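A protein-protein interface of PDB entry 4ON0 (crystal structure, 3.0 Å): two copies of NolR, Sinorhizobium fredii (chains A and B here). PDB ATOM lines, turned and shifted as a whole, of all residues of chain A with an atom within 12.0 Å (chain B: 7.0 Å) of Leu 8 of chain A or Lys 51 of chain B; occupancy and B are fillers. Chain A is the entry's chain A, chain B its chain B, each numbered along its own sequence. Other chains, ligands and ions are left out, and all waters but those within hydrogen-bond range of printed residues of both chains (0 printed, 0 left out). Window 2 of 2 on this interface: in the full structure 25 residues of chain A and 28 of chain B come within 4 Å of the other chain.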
ATOM      1  N   GLN A   6      18.175  -3.507   9.302  1.00  0.00           N
ATOM      2  CA  GLN A   6      18.445  -2.237   8.643  1.00  0.00           C
ATOM      3  C   GLN A   6      19.826  -1.773   9.187  1.00  0.00           C
ATOM      4  O   GLN A   6      20.302  -2.341  10.165  1.00  0.00           O
ATOM      5  CB  GLN A   6      17.275  -1.231   8.857  1.00  0.00           C
ATOM      6  CG  GLN A   6      17.268  -0.295  10.101  1.00  0.00           C
ATOM      7  CD  GLN A   6      17.143  -0.967  11.460  1.00  0.00           C
ATOM      8  OE1 GLN A   6      16.691  -2.112  11.575  1.00  0.00           O
ATOM      9  NE2 GLN A   6      17.567  -0.251  12.509  1.00  0.00           N
ATOM     10  N   PRO A   7      20.469  -0.752   8.581  1.00  0.00           N
ATOM     11  CA  PRO A   7      21.944  -0.813   8.492  1.00  0.00           C
ATOM     12  C   PRO A   7      22.787  -0.938   9.767  1.00  0.00           C
ATOM     13  O   PRO A   7      22.344  -0.681  10.889  1.00  0.00           O
ATOM     14  CB  PRO A   7      22.305   0.520   7.833  1.00  0.00           C
ATOM     15  CG  PRO A   7      21.115   0.919   7.092  1.00  0.00           C
ATOM     16  CD  PRO A   7      19.946   0.457   7.920  1.00  0.00           C
ATOM     17  N   LEU A   8      24.042  -1.325   9.542  1.00  0.00           N
ATOM     18  CA  LEU A   8      25.036  -1.517  10.591  1.00  0.00           C
ATOM     19  C   LEU A   8      25.477  -0.185  11.183  1.00  0.00           C
ATOM     20  O   LEU A   8      25.574   0.820  10.481  1.00  0.00           O
ATOM     21  CB  LEU A   8      26.257  -2.254  10.032  1.00  0.00           C
ATOM     22  CG  LEU A   8      26.069  -3.717   9.632  1.00  0.00           C
ATOM     23  CD1 LEU A   8      27.349  -4.285   9.037  1.00  0.00           C
ATOM     24  CD2 LEU A   8      25.621  -4.539  10.826  1.00  0.00           C
ATOM     25  N   SER A   9      25.754  -0.194  12.483  1.00  0.00           N
ATOM     26  CA  SER A   9      26.183   0.998  13.206  1.00  0.00           C
ATOM     27  C   SER A   9      27.608   1.407  12.848  1.00  0.00           C
ATOM     28  O   SER A   9      28.465   0.547  12.647  1.00  0.00           O
ATOM     29  CB  SER A   9      26.076   0.764  14.714  1.00  0.00           C
ATOM     30  OG  SER A   9      27.057  -0.158  15.155  1.00  0.00           O
ATOM     31  N   PRO A  10      27.857   2.726  12.739  1.00  0.00           N
ATOM     32  CA  PRO A  10      29.160   3.278  12.342  1.00  0.00           C
ATOM     33  C   PRO A  10      30.313   2.697  13.166  1.00  0.00           C
ATOM     34  O   PRO A  10      31.454   2.655  12.695  1.00  0.00           O
ATOM     35  CB  PRO A  10      29.000   4.774  12.612  1.00  0.00           C
ATOM     36  CG  PRO A  10      27.542   5.022  12.435  1.00  0.00           C
ATOM     37  CD  PRO A  10      26.856   3.788  12.956  1.00  0.00           C
ATOM     38  N   GLU A  11      30.001   2.258  14.383  1.00  0.00           N
ATOM     39  CA  GLU A  11      30.964   1.591  15.254  1.00  0.00           C
ATOM     40  C   GLU A  11      31.449   0.294  14.624  1.00  0.00           C
ATOM     41  O   GLU A  11      32.640  -0.024  14.640  1.00  0.00           O
ATOM     42  CB  GLU A  11      30.337   1.292  16.615  1.00  0.00           C
ATOM     43  CG  GLU A  11      29.902   2.522  17.389  1.00  0.00           C
ATOM     44  CD  GLU A  11      28.442   2.463  17.785  1.00  0.00           C
ATOM     45  OE1 GLU A  11      27.772   1.467  17.436  1.00  0.00           O
ATOM     46  OE2 GLU A  11      27.964   3.409  18.445  1.00  0.00           O
ATOM     47  N   LYS A  12      30.502  -0.452  14.068  1.00  0.00           N
ATOM     48  CA  LYS A  12      30.816  -1.674  13.349  1.00  0.00           C
ATOM     49  C   LYS A  12      31.675  -1.367  12.128  1.00  0.00           C
ATOM     50  O   LYS A  12      32.630  -2.091  11.844  1.00  0.00           O
ATOM     51  CB  LYS A  12      29.532  -2.397  12.947  1.00  0.00           C
ATOM     52  CG  LYS A  12      28.672  -2.805  14.137  1.00  0.00           C
ATOM     53  CD  LYS A  12      27.243  -3.129  13.728  1.00  0.00           C
ATOM     54  CE  LYS A  12      26.377  -3.405  14.950  1.00  0.00           C
ATOM     55  NZ  LYS A  12      24.943  -3.582  14.593  1.00  0.00           N
ATOM     56  N   HIS A  13      31.333  -0.299  11.411  1.00  0.00           N
ATOM     57  CA  HIS A  13      32.143   0.160  10.285  1.00  0.00           C
ATOM     58  C   HIS A  13      33.580   0.433  10.679  1.00  0.00           C
ATOM     59  O   HIS A  13      34.502   0.072   9.960  1.00  0.00           O
ATOM     60  CB  HIS A  13      31.542   1.419   9.661  1.00  0.00           C
ATOM     61  CG  HIS A  13      30.468   1.138   8.660  1.00  0.00           C
ATOM     62  ND1 HIS A  13      29.272   0.540   8.996  1.00  0.00           N
ATOM     63  CD2 HIS A  13      30.416   1.354   7.324  1.00  0.00           C
ATOM     64  CE1 HIS A  13      28.527   0.411   7.914  1.00  0.00           C
ATOM     65  NE2 HIS A  13      29.197   0.897   6.885  1.00  0.00           N
ATOM     66  N   GLU A  14      33.762   1.088  11.822  1.00  0.00           N
ATOM     67  CA  GLU A  14      35.104   1.398  12.316  1.00  0.00           C
ATOM     68  C   GLU A  14      35.873   0.137  12.725  1.00  0.00           C
ATOM     69  O   GLU A  14      37.061  -0.002  12.396  1.00  0.00           O
ATOM     70  CB  GLU A  14      35.040   2.400  13.471  1.00  0.00           C
ATOM     71  CG  GLU A  14      34.843   3.826  12.983  1.00  0.00           C
ATOM     72  CD  GLU A  14      36.117   4.401  12.380  1.00  0.00           C
ATOM     73  OE1 GLU A  14      36.032   5.366  11.594  1.00  0.00           O
ATOM     74  OE2 GLU A  14      37.184   3.783  12.570  1.00  0.00           O
ATOM     75  N   GLU A  15      35.207  -0.762  13.450  1.00  0.00           N
ATOM     76  CA  GLU A  15      35.788  -2.053  13.813  1.00  0.00           C
ATOM     77  C   GLU A  15      36.285  -2.758  12.551  1.00  0.00           C
ATOM     78  O   GLU A  15      37.417  -3.258  12.489  1.00  0.00           O
ATOM     79  CB  GLU A  15      34.744  -2.912  14.529  1.00  0.00           C
ATOM     80  CG  GLU A  15      34.373  -2.408  15.911  1.00  0.00           C
ATOM     81  CD  GLU A  15      33.318  -3.262  16.590  1.00  0.00           C
ATOM     82  OE1 GLU A  15      33.113  -4.417  16.156  1.00  0.00           O
ATOM     83  OE2 GLU A  15      32.671  -2.766  17.539  1.00  0.00           O
ATOM     84  N   ALA A  16      35.424  -2.774  11.539  1.00  0.00           N
ATOM     85  CA  ALA A  16      35.754  -3.373  10.259  1.00  0.00           C
ATOM     86  C   ALA A  16      36.936  -2.672   9.606  1.00  0.00           C
ATOM     87  O   ALA A  16      37.779  -3.323   9.003  1.00  0.00           O
ATOM     88  CB  ALA A  16      34.548  -3.349   9.331  1.00  0.00           C
ATOM     89  N   GLU A  17      36.998  -1.350   9.737  1.00  0.00           N
ATOM     90  CA  GLU A  17      38.082  -0.568   9.150  1.00  0.00           C
ATOM     91  C   GLU A  17      39.424  -0.955   9.754  1.00  0.00           C
ATOM     92  O   GLU A  17      40.393  -1.191   9.032  1.00  0.00           O
ATOM     93  CB  GLU A  17      37.831   0.932   9.341  1.00  0.00           C
ATOM     94  CG  GLU A  17      36.991   1.576   8.247  1.00  0.00           C
ATOM     95  CD  GLU A  17      37.794   1.886   6.994  1.00  0.00           C
ATOM     96  OE1 GLU A  17      39.021   1.643   6.990  1.00  0.00           O
ATOM     97  OE2 GLU A  17      37.198   2.371   6.009  1.00  0.00           O
ATOM     98  N   LEU B  33      32.464  -7.035   6.721  1.00  0.00           N
ATOM     99  CA  LEU B  33      31.083  -6.931   7.185  1.00  0.00           C
ATOM    100  C   LEU B  33      30.205  -7.933   6.441  1.00  0.00           C
ATOM    101  O   LEU B  33      29.377  -8.637   7.042  1.00  0.00           O
ATOM    102  CB  LEU B  33      30.552  -5.511   6.989  1.00  0.00           C
ATOM    103  CG  LEU B  33      31.302  -4.402   7.727  1.00  0.00           C
ATOM    104  CD1 LEU B  33      30.851  -3.033   7.245  1.00  0.00           C
ATOM    105  CD2 LEU B  33      31.097  -4.537   9.228  1.00  0.00           C
ATOM    106  N   ILE B  34      30.403  -7.991   5.127  1.00  0.00           N
ATOM    107  CA  ILE B  34      29.690  -8.931   4.278  1.00  0.00           C
ATOM    108  C   ILE B  34      29.868 -10.359   4.772  1.00  0.00           C
ATOM    109  O   ILE B  34      28.889 -11.056   5.018  1.00  0.00           O
ATOM    110  CB  ILE B  34      30.170  -8.847   2.818  1.00  0.00           C
ATOM    111  CG1 ILE B  34      29.740  -7.524   2.188  1.00  0.00           C
ATOM    112  CG2 ILE B  34      29.614 -10.003   2.007  1.00  0.00           C
ATOM    113  CD1 ILE B  34      30.330  -7.292   0.820  1.00  0.00           C
ATOM    114  N   ASP B  36      30.892 -11.490   7.650  1.00  0.00           N
ATOM    115  CA  ASP B  36      30.275 -11.647   8.964  1.00  0.00           C
ATOM    116  C   ASP B  36      28.782 -11.961   8.813  1.00  0.00           C
ATOM    117  O   ASP B  36      28.280 -13.012   9.271  1.00  0.00           O
ATOM    118  CB  ASP B  36      30.481 -10.386   9.803  1.00  0.00           C
ATOM    119  CG  ASP B  36      29.923 -10.519  11.205  1.00  0.00           C
ATOM    120  OD1 ASP B  36      30.623 -11.082  12.076  1.00  0.00           O
ATOM    121  OD2 ASP B  36      28.786 -10.059  11.437  1.00  0.00           O
ATOM    122  N   SER B  37      28.083 -11.039   8.158  1.00  0.00           N
ATOM    123  CA  SER B  37      26.642 -11.149   7.962  1.00  0.00           C
ATOM    124  C   SER B  37      26.225 -12.439   7.244  1.00  0.00           C
ATOM    125  O   SER B  37      25.230 -13.063   7.611  1.00  0.00           O
ATOM    126  CB  SER B  37      26.130  -9.936   7.187  1.00  0.00           C
ATOM    127  OG  SER B  37      26.453  -8.731   7.859  1.00  0.00           O
ATOM    128  N   GLU B  41      23.856 -15.537   8.450  1.00  0.00           N
ATOM    129  CA  GLU B  41      22.574 -15.790   7.789  1.00  0.00           C
ATOM    130  C   GLU B  41      22.598 -15.688   6.265  1.00  0.00           C
ATOM    131  O   GLU B  41      23.534 -15.152   5.674  1.00  0.00           O
ATOM    132  CB  GLU B  41      21.511 -14.830   8.342  1.00  0.00           C
ATOM    133  CG  GLU B  41      21.862 -13.359   8.217  1.00  0.00           C
ATOM    134  CD  GLU B  41      20.787 -12.458   8.802  1.00  0.00           C
ATOM    135  OE1 GLU B  41      21.011 -11.233   8.885  1.00  0.00           O
ATOM    136  OE2 GLU B  41      19.718 -12.976   9.186  1.00  0.00           O
ATOM    137  N   MET B  43      21.147 -13.992   2.901  1.00  0.00           N
ATOM    138  CA  MET B  43      20.613 -12.678   2.576  1.00  0.00           C
ATOM    139  C   MET B  43      20.523 -12.431   1.080  1.00  0.00           C
ATOM    140  O   MET B  43      21.334 -12.931   0.299  1.00  0.00           O
ATOM    141  CB  MET B  43      21.455 -11.582   3.222  1.00  0.00           C
ATOM    142  CG  MET B  43      20.836 -11.005   4.476  1.00  0.00           C
ATOM    143  SD  MET B  43      21.735  -9.567   5.077  1.00  0.00           S
ATOM    144  CE  MET B  43      22.770 -10.328   6.318  1.00  0.00           C
ATOM    145  N   VAL B  45      20.760  -9.873  -2.173  1.00  0.00           N
ATOM    146  CA  VAL B  45      21.768  -8.874  -2.493  1.00  0.00           C
ATOM    147  C   VAL B  45      21.310  -7.469  -2.093  1.00  0.00           C
ATOM    148  O   VAL B  45      22.095  -6.691  -1.560  1.00  0.00           O
ATOM    149  CB  VAL B  45      22.133  -8.919  -3.986  1.00  0.00           C
ATOM    150  CG1 VAL B  45      23.063  -7.775  -4.350  1.00  0.00           C
ATOM    151  CG2 VAL B  45      22.779 -10.257  -4.314  1.00  0.00           C
ATOM    152  N   GLY B  46      20.038  -7.154  -2.325  1.00  0.00           N
ATOM    153  CA  GLY B  46      19.505  -5.853  -1.950  1.00  0.00           C
ATOM    154  C   GLY B  46      19.610  -5.599  -0.455  1.00  0.00           C
ATOM    155  O   GLY B  46      20.067  -4.535  -0.011  1.00  0.00           O
ATOM    156  N   ALA B  47      19.191  -6.592   0.325  1.00  0.00           N
ATOM    157  CA  ALA B  47      19.243  -6.509   1.780  1.00  0.00           C
ATOM    158  C   ALA B  47      20.679  -6.316   2.260  1.00  0.00           C
ATOM    159  O   ALA B  47      20.931  -5.547   3.184  1.00  0.00           O
ATOM    160  CB  ALA B  47      18.637  -7.752   2.402  1.00  0.00           C
ATOM    161  N   LEU B  48      21.609  -7.023   1.627  1.00  0.00           N
ATOM    162  CA  LEU B  48      23.027  -6.865   1.921  1.00  0.00           C
ATOM    163  C   LEU B  48      23.448  -5.426   1.653  1.00  0.00           C
ATOM    164  O   LEU B  48      24.170  -4.812   2.439  1.00  0.00           O
ATOM    165  CB  LEU B  48      23.871  -7.826   1.084  1.00  0.00           C
ATOM    166  CG  LEU B  48      24.581  -8.957   1.828  1.00  0.00           C
ATOM    167  CD1 LEU B  48      25.410  -9.779   0.857  1.00  0.00           C
ATOM    168  CD2 LEU B  48      25.446  -8.408   2.948  1.00  0.00           C
ATOM    169  N   ALA B  49      22.984  -4.902   0.524  1.00  0.00           N
ATOM    170  CA  ALA B  49      23.273  -3.537   0.106  1.00  0.00           C
ATOM    171  C   ALA B  49      22.791  -2.532   1.147  1.00  0.00           C
ATOM    172  O   ALA B  49      23.423  -1.495   1.349  1.00  0.00           O
ATOM    173  CB  ALA B  49      22.645  -3.252  -1.253  1.00  0.00           C
ATOM    174  N   ASN B  50      21.671  -2.829   1.802  1.00  0.00           N
ATOM    175  CA  ASN B  50      21.184  -1.933   2.849  1.00  0.00           C
ATOM    176  C   ASN B  50      21.816  -2.240   4.199  1.00  0.00           C
ATOM    177  O   ASN B  50      21.710  -1.447   5.131  1.00  0.00           O
ATOM    178  CB  ASN B  50      19.665  -2.046   3.010  1.00  0.00           C
ATOM    179  CG  ASN B  50      18.923  -1.846   1.714  1.00  0.00           C
ATOM    180  OD1 ASN B  50      19.346  -1.078   0.849  1.00  0.00           O
ATOM    181  ND2 ASN B  50      17.815  -2.561   1.560  1.00  0.00           N
ATOM    182  N   LYS B  51      22.479  -3.386   4.305  1.00  0.00           N
ATOM    183  CA  LYS B  51      23.128  -3.750   5.558  1.00  0.00           C
ATOM    184  C   LYS B  51      24.565  -3.246   5.691  1.00  0.00           C
ATOM    185  O   LYS B  51      25.003  -2.911   6.789  1.00  0.00           O
ATOM    186  CB  LYS B  51      23.094  -5.277   5.710  1.00  0.00           C
ATOM    187  CG  LYS B  51      23.687  -5.819   7.000  1.00  0.00           C
ATOM    188  CD  LYS B  51      22.680  -5.800   8.137  1.00  0.00           C
ATOM    189  CE  LYS B  51      23.178  -6.620   9.316  1.00  0.00           C
ATOM    190  NZ  LYS B  51      22.234  -6.591  10.466  1.00  0.00           N
ATOM    191  N   VAL B  52      25.289  -3.164   4.579  1.00  0.00           N
ATOM    192  CA  VAL B  52      26.632  -2.587   4.602  1.00  0.00           C
ATOM    193  C   VAL B  52      26.670  -1.169   4.033  1.00  0.00           C
ATOM    194  O   VAL B  52      27.736  -0.557   3.947  1.00  0.00           O
ATOM    195  CB  VAL B  52      27.643  -3.470   3.840  1.00  0.00           C
ATOM    196  CG1 VAL B  52      27.665  -4.875   4.425  1.00  0.00           C
ATOM    197  CG2 VAL B  52      27.317  -3.502   2.359  1.00  0.00           C
ATOM    198  N   GLY B  53      25.506  -0.654   3.645  1.00  0.00           N
ATOM    199  CA  GLY B  53      25.404   0.688   3.101  1.00  0.00           C
ATOM    200  C   GLY B  53      26.191   0.844   1.814  1.00  0.00           C
ATOM    201  O   GLY B  53      26.960   1.792   1.649  1.00  0.00           O
ATOM    202  N   LEU B  54      25.995  -0.095   0.896  1.00  0.00           N
ATOM    203  CA  LEU B  54      26.708  -0.085  -0.372  1.00  0.00           C
ATOM    204  C   LEU B  54      25.725  -0.120  -1.538  1.00  0.00           C
ATOM    205  O   LEU B  54      24.614  -0.633  -1.408  1.00  0.00           O
ATOM    206  CB  LEU B  54      27.673  -1.268  -0.444  1.00  0.00           C
ATOM    207  CG  LEU B  54      28.837  -1.178  -1.428  1.00  0.00           C
ATOM    208  CD1 LEU B  54      29.600   0.122  -1.234  1.00  0.00           C
ATOM    209  CD2 LEU B  54      29.765  -2.370  -1.247  1.00  0.00           C
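No position is printed for both chains.
Of the 6 pairs that touch across the chains among the printed residues, none has its exchanged pair printed and touching as well.
Pro 7 of chain A touches Asn 50 of chain B (CG to O, 3.1 Å).
Leu 33 of chain B touches Leu 8 of chain A.
Lys 12 of chain A touches Leu 33 of chain B.
Val 52 of chain B touches His 13 of chain A (O to NE2, 3.6 Å).
Ala 16 of chain A touches Leu 33 of chain B (CB to CD2, 3.7 Å).
The side-chain amide nitrogen (ND2) of Asn 50 of chain B lies within hydrogen-bond range of the backbone carbonyl oxygen (O) of Gly 46 of chain B (3.4 Å).
The backbone carbonyl oxygen (O) of Leu 33 of chain B lies within hydrogen-bond range of the side-chain hydroxyl (OG) of Ser 37 of chain B (3.0 Å).
O of Lys 51 of chain B lies close to N of Leu 8 of chain A.
Leu 8 of chain A touches two residues of chain B.
Lys 51 of chain B touches one residue of chain A.
No residue of chain A comes within 4 Å of Ser 37 of chain B.
No residue of chain A comes within 4 Å of Ala 47 of chain B.
Asn 50 of chain B touches just one residue of chain A: Pro 7 (3.1 Å).
Val 52 of chain B touches just one residue of chain A: His 13.
No residue of chain A comes within 4 Å of Gly 53 of chain B.
Of the printed residues of chain B, His 13 of chain A touches Val 52 (3.6 Å).
Printed residues of chain B within 4 Å of Ala 16 of chain A: Leu 33.
Of the printed residues of chain B, Pro 7 of chain A touches Asn 50.
Val 45 of chain B touches none of the printed residues of chain A.
Of the 16 printed residues of chain B, 4 touch a printed residue of chain A.
Printed residues of chain B that touch a printed residue of chain A: Leu 33, Asn 50, Lys 51 and Val 52.
Among the printed residues, 6 pairs touch across the chains.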
